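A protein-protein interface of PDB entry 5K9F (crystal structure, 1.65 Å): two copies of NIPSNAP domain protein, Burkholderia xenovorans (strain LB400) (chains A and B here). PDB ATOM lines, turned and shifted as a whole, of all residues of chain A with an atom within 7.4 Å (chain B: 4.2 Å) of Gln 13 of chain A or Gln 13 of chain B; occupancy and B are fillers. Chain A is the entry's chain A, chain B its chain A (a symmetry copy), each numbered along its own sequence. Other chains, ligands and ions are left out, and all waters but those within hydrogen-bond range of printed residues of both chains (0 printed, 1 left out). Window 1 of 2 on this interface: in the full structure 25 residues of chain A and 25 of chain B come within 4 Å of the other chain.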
ATOM      1  N   VAL A  11      14.369 -29.071 -17.889  1.00  0.00           N
ATOM      2  CA  VAL A  11      14.225 -28.264 -16.683  1.00  0.00           C
ATOM      3  C   VAL A  11      15.204 -27.102 -16.729  1.00  0.00           C
ATOM      4  O   VAL A  11      16.394 -27.285 -17.017  1.00  0.00           O
ATOM      5  CB  VAL A  11      14.418 -29.121 -15.420  1.00  0.00           C
ATOM      6  CG1 VAL A  11      14.412 -28.255 -14.197  1.00  0.00           C
ATOM      7  CG2 VAL A  11      13.296 -30.155 -15.322  1.00  0.00           C
ATOM      8  N   GLU A  12      14.705 -25.901 -16.467  1.00  0.00           N
ATOM      9  CA  GLU A  12      15.559 -24.724 -16.390  1.00  0.00           C
ATOM     10  C   GLU A  12      15.662 -24.259 -14.946  1.00  0.00           C
ATOM     11  O   GLU A  12      14.636 -24.100 -14.272  1.00  0.00           O
ATOM     12  CB  GLU A  12      15.015 -23.593 -17.262  1.00  0.00           C
ATOM     13  CG  GLU A  12      15.875 -22.339 -17.135  1.00  0.00           C
ATOM     14  CD  GLU A  12      15.356 -21.168 -17.964  1.00  0.00           C
ATOM     15  OE1 GLU A  12      14.223 -21.262 -18.479  1.00  0.00           O
ATOM     16  OE2 GLU A  12      16.082 -20.149 -18.085  1.00  0.00           O
ATOM     17  N   GLN A  13      16.893 -24.048 -14.460  1.00  0.00           N
ATOM     18  CA  GLN A  13      17.102 -23.484 -13.125  1.00  0.00           C
ATOM     19  C   GLN A  13      17.712 -22.101 -13.300  1.00  0.00           C
ATOM     20  O   GLN A  13      18.850 -21.975 -13.765  1.00  0.00           O
ATOM     21  CB  GLN A  13      17.995 -24.360 -12.240  1.00  0.00           C
ATOM     22  CG  GLN A  13      18.138 -23.724 -10.845  1.00  0.00           C
ATOM     23  CD  GLN A  13      18.764 -24.633  -9.802  1.00  0.00           C
ATOM     24  OE1 GLN A  13      18.548 -24.447  -8.609  1.00  0.00           O
ATOM     25  NE2 GLN A  13      19.565 -25.587 -10.241  1.00  0.00           N
ATOM     26  N   ARG A  14      16.962 -21.068 -12.918  1.00  0.00           N
ATOM     27  CA  ARG A  14      17.403 -19.684 -13.056  1.00  0.00           C
ATOM     28  C   ARG A  14      17.745 -19.128 -11.686  1.00  0.00           C
ATOM     29  O   ARG A  14      17.050 -19.401 -10.704  1.00  0.00           O
ATOM     30  CB  ARG A  14      16.321 -18.799 -13.670  1.00  0.00           C
ATOM     31  CG  ARG A  14      15.958 -19.143 -15.060  1.00  0.00           C
ATOM     32  CD  ARG A  14      14.773 -18.313 -15.509  1.00  0.00           C
ATOM     33  NE  ARG A  14      15.071 -16.908 -15.781  1.00  0.00           N
ATOM     34  CZ  ARG A  14      15.649 -16.461 -16.901  1.00  0.00           C
ATOM     35  NH1 ARG A  14      16.042 -17.304 -17.856  1.00  0.00           N
ATOM     36  NH2 ARG A  14      15.831 -15.169 -17.072  1.00  0.00           N
ATOM     37  N   THR A  15      18.801 -18.330 -11.623  1.00  0.00           N
ATOM     38  CA  THR A  15      19.185 -17.677 -10.378  1.00  0.00           C
ATOM     39  C   THR A  15      19.276 -16.183 -10.627  1.00  0.00           C
ATOM     40  O   THR A  15      19.947 -15.754 -11.569  1.00  0.00           O
ATOM     41  CB  THR A  15      20.540 -18.185  -9.849  1.00  0.00           C
ATOM     42  OG1 THR A  15      20.490 -19.591  -9.577  1.00  0.00           O
ATOM     43  CG2 THR A  15      20.937 -17.459  -8.556  1.00  0.00           C
ATOM     44  N   TYR A  49      12.339 -20.298  -4.884  1.00  0.00           N
ATOM     45  CA  TYR A  49      12.990 -20.295  -3.578  1.00  0.00           C
ATOM     46  C   TYR A  49      13.811 -19.031  -3.370  1.00  0.00           C
ATOM     47  O   TYR A  49      14.182 -18.337  -4.321  1.00  0.00           O
ATOM     48  CB  TYR A  49      13.953 -21.489  -3.434  1.00  0.00           C
ATOM     49  CG  TYR A  49      13.369 -22.826  -3.783  1.00  0.00           C
ATOM     50  CD1 TYR A  49      12.561 -23.505  -2.871  1.00  0.00           C
ATOM     51  CD2 TYR A  49      13.627 -23.421  -5.012  1.00  0.00           C
ATOM     52  CE1 TYR A  49      12.027 -24.746  -3.185  1.00  0.00           C
ATOM     53  CE2 TYR A  49      13.104 -24.662  -5.331  1.00  0.00           C
ATOM     54  CZ  TYR A  49      12.310 -25.318  -4.415  1.00  0.00           C
ATOM     55  OH  TYR A  49      11.772 -26.559  -4.724  1.00  0.00           O
ATOM     56  N   ARG A  58      19.657 -14.398  -3.089  1.00  0.00           N
ATOM     57  CA  ARG A  58      19.376 -15.089  -4.336  1.00  0.00           C
ATOM     58  C   ARG A  58      17.936 -15.537  -4.365  1.00  0.00           C
ATOM     59  O   ARG A  58      17.400 -16.008  -3.355  1.00  0.00           O
ATOM     60  CB  ARG A  58      20.243 -16.337  -4.509  1.00  0.00           C
ATOM     61  CG  ARG A  58      21.690 -16.069  -4.847  1.00  0.00           C
ATOM     62  CD  ARG A  58      22.408 -17.406  -5.025  1.00  0.00           C
ATOM     63  NE  ARG A  58      22.539 -18.126  -3.752  1.00  0.00           N
ATOM     64  CZ  ARG A  58      22.619 -19.448  -3.637  1.00  0.00           C
ATOM     65  NH1 ARG A  58      22.566 -20.230  -4.715  1.00  0.00           N
ATOM     66  NH2 ARG A  58      22.761 -19.994  -2.427  1.00  0.00           N
ATOM     67  N   ILE A  60      15.817 -18.332  -6.699  1.00  0.00           N
ATOM     68  CA  ILE A  60      16.126 -19.477  -7.539  1.00  0.00           C
ATOM     69  C   ILE A  60      14.813 -20.071  -8.008  1.00  0.00           C
ATOM     70  O   ILE A  60      13.935 -20.363  -7.185  1.00  0.00           O
ATOM     71  CB  ILE A  60      16.957 -20.511  -6.763  1.00  0.00           C
ATOM     72  CG1 ILE A  60      18.311 -19.900  -6.382  1.00  0.00           C
ATOM     73  CG2 ILE A  60      17.159 -21.765  -7.580  1.00  0.00           C
ATOM     74  CD1 ILE A  60      19.063 -20.769  -5.394  1.00  0.00           C
ATOM     75  N   GLN A  61      14.660 -20.232  -9.327  1.00  0.00           N
ATOM     76  CA  GLN A  61      13.412 -20.771  -9.846  1.00  0.00           C
ATOM     77  C   GLN A  61      13.681 -21.937 -10.782  1.00  0.00           C
ATOM     78  O   GLN A  61      14.653 -21.937 -11.534  1.00  0.00           O
ATOM     79  CB  GLN A  61      12.580 -19.697 -10.566  1.00  0.00           C
ATOM     80  CG  GLN A  61      13.309 -18.889 -11.589  1.00  0.00           C
ATOM     81  CD  GLN A  61      12.566 -17.618 -11.931  1.00  0.00           C
ATOM     82  OE1 GLN A  61      11.720 -17.608 -12.816  1.00  0.00           O
ATOM     83  NE2 GLN A  61      12.873 -16.538 -11.217  1.00  0.00           N
ATOM     84  N   LEU A  62      12.818 -22.943 -10.717  1.00  0.00           N
ATOM     85  CA  LEU A  62      12.892 -24.085 -11.613  1.00  0.00           C
ATOM     86  C   LEU A  62      11.607 -24.158 -12.420  1.00  0.00           C
ATOM     87  O   LEU A  62      10.511 -24.101 -11.860  1.00  0.00           O
ATOM     88  CB  LEU A  62      13.114 -25.394 -10.851  1.00  0.00           C
ATOM     89  CG  LEU A  62      14.543 -25.557 -10.319  1.00  0.00           C
ATOM     90  CD1 LEU A  62      14.711 -24.877  -8.971  1.00  0.00           C
ATOM     91  CD2 LEU A  62      14.907 -27.030 -10.237  1.00  0.00           C
ATOM     92  N   TRP A  63      11.759 -24.280 -13.736  1.00  0.00           N
ATOM     93  CA  TRP A  63      10.644 -24.376 -14.677  1.00  0.00           C
ATOM     94  C   TRP A  63      10.806 -25.623 -15.529  1.00  0.00           C
ATOM     95  O   TRP A  63      11.919 -25.956 -15.942  1.00  0.00           O
ATOM     96  CB  TRP A  63      10.594 -23.151 -15.605  1.00  0.00           C
ATOM     97  CG  TRP A  63      10.337 -21.860 -14.900  1.00  0.00           C
ATOM     98  CD1 TRP A  63      11.270 -20.995 -14.409  1.00  0.00           C
ATOM     99  CD2 TRP A  63       9.059 -21.292 -14.598  1.00  0.00           C
ATOM    100  NE1 TRP A  63      10.645 -19.910 -13.823  1.00  0.00           N
ATOM    101  CE2 TRP A  63       9.291 -20.079 -13.919  1.00  0.00           C
ATOM    102  CE3 TRP A  63       7.737 -21.699 -14.825  1.00  0.00           C
ATOM    103  CZ2 TRP A  63       8.248 -19.260 -13.480  1.00  0.00           C
ATOM    104  CZ3 TRP A  63       6.708 -20.886 -14.394  1.00  0.00           C
ATOM    105  CH2 TRP A  63       6.973 -19.685 -13.720  1.00  0.00           C
ATOM    106  N   PHE A  65       9.745 -27.664 -19.050  1.00  0.00           N
ATOM    107  CA  PHE A  65       9.285 -27.456 -20.419  1.00  0.00           C
ATOM    108  C   PHE A  65       9.238 -28.773 -21.177  1.00  0.00           C
ATOM    109  O   PHE A  65      10.060 -29.665 -20.954  1.00  0.00           O
ATOM    110  CB  PHE A  65      10.195 -26.479 -21.163  1.00  0.00           C
ATOM    111  CG  PHE A  65      10.226 -25.111 -20.557  1.00  0.00           C
ATOM    112  CD1 PHE A  65       9.207 -24.209 -20.807  1.00  0.00           C
ATOM    113  CD2 PHE A  65      11.292 -24.715 -19.756  1.00  0.00           C
ATOM    114  CE1 PHE A  65       9.234 -22.926 -20.260  1.00  0.00           C
ATOM    115  CE2 PHE A  65      11.321 -23.444 -19.194  1.00  0.00           C
ATOM    116  CZ  PHE A  65      10.299 -22.547 -19.450  1.00  0.00           C
ATOM    117  N   SER A  99      21.616 -15.701 -13.946  1.00  0.00           N
ATOM    118  CA  SER A  99      22.226 -16.861 -14.582  1.00  0.00           C
ATOM    119  C   SER A  99      21.172 -17.938 -14.776  1.00  0.00           C
ATOM    120  O   SER A  99      20.140 -17.946 -14.115  1.00  0.00           O
ATOM    121  CB  SER A  99      23.387 -17.421 -13.757  1.00  0.00           C
ATOM    122  OG  SER A  99      22.894 -18.018 -12.571  1.00  0.00           O
ATOM    123  N   THR A 100      21.443 -18.858 -15.705  1.00  0.00           N
ATOM    124  CA  THR A 100      20.517 -19.970 -15.880  1.00  0.00           C
ATOM    125  C   THR A 100      21.260 -21.209 -16.371  1.00  0.00           C
ATOM    126  O   THR A 100      22.374 -21.138 -16.892  1.00  0.00           O
ATOM    127  CB  THR A 100      19.379 -19.613 -16.830  1.00  0.00           C
ATOM    128  OG1 THR A 100      18.349 -20.602 -16.692  1.00  0.00           O
ATOM    129  CG2 THR A 100      19.861 -19.563 -18.290  1.00  0.00           C
ATOM    130  N   GLU A 101      20.632 -22.364 -16.175  1.00  0.00           N
ATOM    131  CA  GLU A 101      21.225 -23.621 -16.615  1.00  0.00           C
ATOM    132  C   GLU A 101      20.108 -24.569 -17.014  1.00  0.00           C
ATOM    133  O   GLU A 101      18.977 -24.454 -16.535  1.00  0.00           O
ATOM    134  CB  GLU A 101      22.082 -24.260 -15.516  1.00  0.00           C
ATOM    135  CG  GLU A 101      21.259 -24.667 -14.282  1.00  0.00           C
ATOM    136  CD  GLU A 101      22.116 -25.144 -13.111  1.00  0.00           C
ATOM    137  OE1 GLU A 101      23.353 -25.150 -13.229  1.00  0.00           O
ATOM    138  OE2 GLU A 101      21.541 -25.508 -12.069  1.00  0.00           O
ATOM    139  N   LEU A 102      20.429 -25.504 -17.904  1.00  0.00           N
ATOM    140  CA  LEU A 102      19.457 -26.503 -18.332  1.00  0.00           C
ATOM    141  C   LEU A 102      19.822 -27.847 -17.731  1.00  0.00           C
ATOM    142  O   LEU A 102      21.004 -28.218 -17.685  1.00  0.00           O
ATOM    143  CB  LEU A 102      19.396 -26.602 -19.861  1.00  0.00           C
ATOM    144  CG  LEU A 102      19.038 -25.307 -20.586  1.00  0.00           C
ATOM    145  CD1 LEU A 102      19.135 -25.519 -22.093  1.00  0.00           C
ATOM    146  CD2 LEU A 102      17.647 -24.822 -20.207  1.00  0.00           C
ATOM    147  N   LEU A 103      18.797 -28.549 -17.238  1.00  0.00           N
ATOM    148  CA  LEU A 103      18.940 -29.818 -16.533  1.00  0.00           C
ATOM    149  C   LEU A 103      18.010 -30.862 -17.132  1.00  0.00           C
ATOM    150  O   LEU A 103      16.945 -30.536 -17.658  1.00  0.00           O
ATOM    151  CB  LEU A 103      18.589 -29.663 -15.055  1.00  0.00           C
ATOM    152  CG  LEU A 103      19.301 -28.549 -14.285  1.00  0.00           C
ATOM    153  CD1 LEU A 103      18.743 -28.460 -12.854  1.00  0.00           C
ATOM    154  CD2 LEU A 103      20.826 -28.758 -14.269  1.00  0.00           C
ATOM    155  N   VAL B  11      14.343 -26.741   2.147  1.00  0.00           N
ATOM    156  CA  VAL B  11      14.752 -27.428   0.927  1.00  0.00           C
ATOM    157  C   VAL B  11      16.270 -27.457   0.844  1.00  0.00           C
ATOM    158  O   VAL B  11      16.936 -26.431   1.037  1.00  0.00           O
ATOM    159  CB  VAL B  11      14.127 -26.767  -0.314  1.00  0.00           C
ATOM    160  CG1 VAL B  11      14.669 -27.389  -1.565  1.00  0.00           C
ATOM    161  CG2 VAL B  11      12.608 -26.932  -0.276  1.00  0.00           C
ATOM    162  N   GLU B  12      16.823 -28.633   0.580  1.00  0.00           N
ATOM    163  CA  GLU B  12      18.259 -28.769   0.385  1.00  0.00           C
ATOM    164  C   GLU B  12      18.553 -29.055  -1.080  1.00  0.00           C
ATOM    165  O   GLU B  12      17.944 -29.956  -1.670  1.00  0.00           O
ATOM    166  CB  GLU B  12      18.827 -29.890   1.256  1.00  0.00           C
ATOM    167  CG  GLU B  12      20.321 -30.076   1.007  1.00  0.00           C
ATOM    168  CD  GLU B  12      20.932 -31.205   1.832  1.00  0.00           C
ATOM    169  OE1 GLU B  12      20.163 -31.974   2.445  1.00  0.00           O
ATOM    170  OE2 GLU B  12      22.183 -31.326   1.851  1.00  0.00           O
ATOM    171  N   GLN B  13      19.476 -28.288  -1.676  1.00  0.00           N
ATOM    172  CA  GLN B  13      19.923 -28.555  -3.045  1.00  0.00           C
ATOM    173  C   GLN B  13      21.375 -29.001  -2.977  1.00  0.00           C
ATOM    174  O   GLN B  13      22.255 -28.211  -2.615  1.00  0.00           O
ATOM    175  CB  GLN B  13      19.773 -27.341  -3.969  1.00  0.00           C
ATOM    176  CG  GLN B  13      20.227 -27.706  -5.394  1.00  0.00           C
ATOM    177  CD  GLN B  13      19.865 -26.678  -6.451  1.00  0.00           C
ATOM    178  OE1 GLN B  13      19.762 -27.008  -7.628  1.00  0.00           O
ATOM    179  NE2 GLN B  13      19.710 -25.430  -6.045  1.00  0.00           N
ATOM    180  N   ARG B  14      21.628 -30.260  -3.333  1.00  0.00           N
ATOM    181  CA  ARG B  14      22.968 -30.835  -3.287  1.00  0.00           C
ATOM    182  C   ARG B  14      23.494 -30.997  -4.701  1.00  0.00           C
ATOM    183  O   ARG B  14      22.750 -31.377  -5.609  1.00  0.00           O
ATOM    184  CB  ARG B  14      22.977 -32.207  -2.617  1.00  0.00           C
ATOM    185  CG  ARG B  14      22.600 -32.200  -1.190  1.00  0.00           C
ATOM    186  CD  ARG B  14      22.485 -33.619  -0.674  1.00  0.00           C
ATOM    187  NE  ARG B  14      23.759 -34.310  -0.482  1.00  0.00           N
ATOM    188  CZ  ARG B  14      24.569 -34.127   0.566  1.00  0.00           C
ATOM    189  NH1 ARG B  14      24.275 -33.240   1.516  1.00  0.00           N
ATOM    190  NH2 ARG B  14      25.673 -34.835   0.671  1.00  0.00           N
ATOM    191  N   ILE B  60      22.404 -33.163  -9.532  1.00  0.00           N
ATOM    192  CA  ILE B  60      21.818 -32.144  -8.679  1.00  0.00           C
ATOM    193  C   ILE B  60      20.552 -32.721  -8.077  1.00  0.00           C
ATOM    194  O   ILE B  60      19.689 -33.219  -8.811  1.00  0.00           O
ATOM    195  CB  ILE B  60      21.519 -30.868  -9.482  1.00  0.00           C
ATOM    196  CG1 ILE B  60      22.832 -30.269 -10.000  1.00  0.00           C
ATOM    197  CG2 ILE B  60      20.779 -29.859  -8.637  1.00  0.00           C
ATOM    198  CD1 ILE B  60      22.587 -29.170 -11.014  1.00  0.00           C
ATOM    199  N   GLN B  61      20.444 -32.679  -6.744  1.00  0.00           N
ATOM    200  CA  GLN B  61      19.266 -33.240  -6.100  1.00  0.00           C
ATOM    201  C   GLN B  61      18.646 -32.234  -5.147  1.00  0.00           C
ATOM    202  O   GLN B  61      19.346 -31.475  -4.480  1.00  0.00           O
ATOM    203  CB  GLN B  61      19.589 -34.546  -5.354  1.00  0.00           C
ATOM    204  CG  GLN B  61      20.761 -34.491  -4.429  1.00  0.00           C
ATOM    205  CD  GLN B  61      21.258 -35.873  -4.074  1.00  0.00           C
ATOM    206  OE1 GLN B  61      20.787 -36.481  -3.121  1.00  0.00           O
ATOM    207  NE2 GLN B  61      22.210 -36.382  -4.854  1.00  0.00           N
ATOM    208  N   LEU B  62      17.319 -32.222  -5.099  1.00  0.00           N
ATOM    209  CA  LEU B  62      16.587 -31.380  -4.169  1.00  0.00           C
ATOM    210  C   LEU B  62      15.759 -32.265  -3.253  1.00  0.00           C
ATOM    211  O   LEU B  62      15.038 -33.147  -3.720  1.00  0.00           O
ATOM    212  CB  LEU B  62      15.684 -30.379  -4.895  1.00  0.00           C
ATOM    213  CG  LEU B  62      16.451 -29.219  -5.541  1.00  0.00           C
ATOM    214  CD1 LEU B  62      16.958 -29.593  -6.923  1.00  0.00           C
ATOM    215  CD2 LEU B  62      15.577 -27.978  -5.597  1.00  0.00           C
ATOM    216  N   THR B 100      26.459 -28.242  -1.025  1.00  0.00           N
ATOM    217  CA  THR B 100      25.033 -28.198  -0.729  1.00  0.00           C
ATOM    218  C   THR B 100      24.630 -26.804  -0.255  1.00  0.00           C
ATOM    219  O   THR B 100      25.457 -25.994   0.165  1.00  0.00           O
ATOM    220  CB  THR B 100      24.636 -29.251   0.300  1.00  0.00           C
ATOM    221  OG1 THR B 100      23.208 -29.379   0.289  1.00  0.00           O
ATOM    222  CG2 THR B 100      25.114 -28.865   1.710  1.00  0.00           C
ATOM    223  N   GLU B 101      23.335 -26.522  -0.352  1.00  0.00           N
ATOM    224  CA  GLU B 101      22.816 -25.232   0.083  1.00  0.00           C
ATOM    225  C   GLU B 101      21.407 -25.431   0.613  1.00  0.00           C
ATOM    226  O   GLU B 101      20.712 -26.375   0.227  1.00  0.00           O
ATOM    227  CB  GLU B 101      22.804 -24.209  -1.059  1.00  0.00           C
ATOM    228  CG  GLU B 101      21.853 -24.607  -2.202  1.00  0.00           C
ATOM    229  CD  GLU B 101      21.957 -23.695  -3.422  1.00  0.00           C
ATOM    230  OE1 GLU B 101      22.772 -22.756  -3.410  1.00  0.00           O
ATOM    231  OE2 GLU B 101      21.219 -23.927  -4.396  1.00  0.00           O
ATOM    232  N   LEU B 103      17.578 -23.785   1.101  1.00  0.00           N
ATOM    233  CA  LEU B 103      16.658 -22.868   0.436  1.00  0.00           C
ATOM    234  C   LEU B 103      15.316 -22.855   1.152  1.00  0.00           C
ATOM    235  O   LEU B 103      14.909 -23.850   1.754  1.00  0.00           O
ATOM    236  CB  LEU B 103      16.419 -23.290  -1.012  1.00  0.00           C
ATOM    237  CG  LEU B 103      17.656 -23.520  -1.882  1.00  0.00           C
ATOM    238  CD1 LEU B 103      17.236 -24.053  -3.262  1.00  0.00           C
ATOM    239  CD2 LEU B 103      18.496 -22.237  -2.019  1.00  0.00           C
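The side-chain amide nitrogen (NE2) of Gln 13 of chain B sits at hydrogen-bond distance from the side-chain amide oxygen (OE1) of Gln 13 of chain A.
NH1 of Arg 58 of chain A lies within salt-bridge range of OE1 of Glu 101 of chain B, 2.9 Å away.
The backbone carbonyl oxygen (O) of Val 11 of chain A lies within hydrogen-bond range of the backbone NH (N) of Leu 103 of chain A (2.7 Å).
The side-chain hydroxyl (OG1) of Thr 100 of chain A sits at hydrogen-bond distance from the backbone carbonyl oxygen (O) of Gln 13 of chain A, 3.3 Å away.
OE2 of Glu 101 of chain A is in hydrogen-bond range of NE2 of Gln 13 of chain A, at 2.7 Å.
The backbone carbonyl oxygen (O) of Ile 60 of chain A lies within hydrogen-bond range of the backbone NH (N) of Tyr 49 of chain A (2.8 Å).
The backbone carbonyl oxygen (O) of Gln 13 of chain B is in hydrogen-bond range of the side-chain hydroxyl (OG1) of Thr 100 of chain B (3.3 Å).
The side-chain amide nitrogen (NE2) of Gln 13 of chain B sits at hydrogen-bond distance from the side-chain carboxylate (OE2) of Glu 101 of chain B.
Among the printed residues, pairs that only touch across the chains: Tyr 49 of chain A with Val 11 of chain B (3.7 Å), Leu 103 of chain A with Ile 60 of chain B (3.7 Å), Ile 60 of chain A with Leu 103 of chain B (3.7 Å), Tyr 49 of chain A with Leu 103 of chain B (3.9 Å), Ile 60 of chain A with Glu 101 of chain B (3.95 Å) and Glu 101 of chain A with Ile 60 of chain B (3.95 Å).
Of the printed residues of chain B, Gln 13 of chain A touches Gln 13 (3.0 Å).
Of the printed residues of chain B, Glu 101 of chain A touches Ile 60.
Of the printed residues of chain B, Tyr 49 of chain A touches Val 11 (3.7 Å) and Leu 103 (3.9 Å).
Printed residues of chain A within 4 Å of Ile 60 of chain B: Glu 101 (3.95 Å) and Leu 103 (3.7 Å).
Printed residues of chain A within 4 Å of Val 11 of chain B: Tyr 49 (3.7 Å).
The nearest printed residue of chain B that does not touch Gln 13 of chain A is Ile 60 of chain B (4.7 Å).
The nearest residue of chain A that does not touch Gln 13 of chain B is Ile 60 of chain A (4.7 Å).
The nearest printed residue of chain A that does not touch Val 11 of chain B is Leu 62 of chain A (7.8 Å).
Printed residues of chain A that touch a printed residue of chain B: Gln 13, Tyr 49, Arg 58, Ile 60, Glu 101 and Leu 103.
Hydrophobic or aromatic side chains of chain A within 4 Å of the printed part of chain B: Tyr 49, Ile 60 and Leu 103.
Along chain A the printed residues that touch a printed residue of chain B span positions 13 to 103.
Among the printed residues, 8 pairs touch across the chains.
Gln 13 of chain B touches its own counterpart, Gln 13 of chain A.
Ile 60 of chain A touches Glu 101 of chain B, and with the chains exchanged Glu 101 of chain A touches Ile 60 of chain B.
Ile 60 of chain A touches Leu 103 of chain B, and with the chains exchanged Leu 103 of chain A touches Ile 60 of chain B.
Positions printed for both chains: 11, 12, 13, 14, 60, 61, 62, 100, 101 and 103.
Of the 8 pairs that touch across the chains among the printed residues, 5 have their exchanged pair printed and touching as well.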
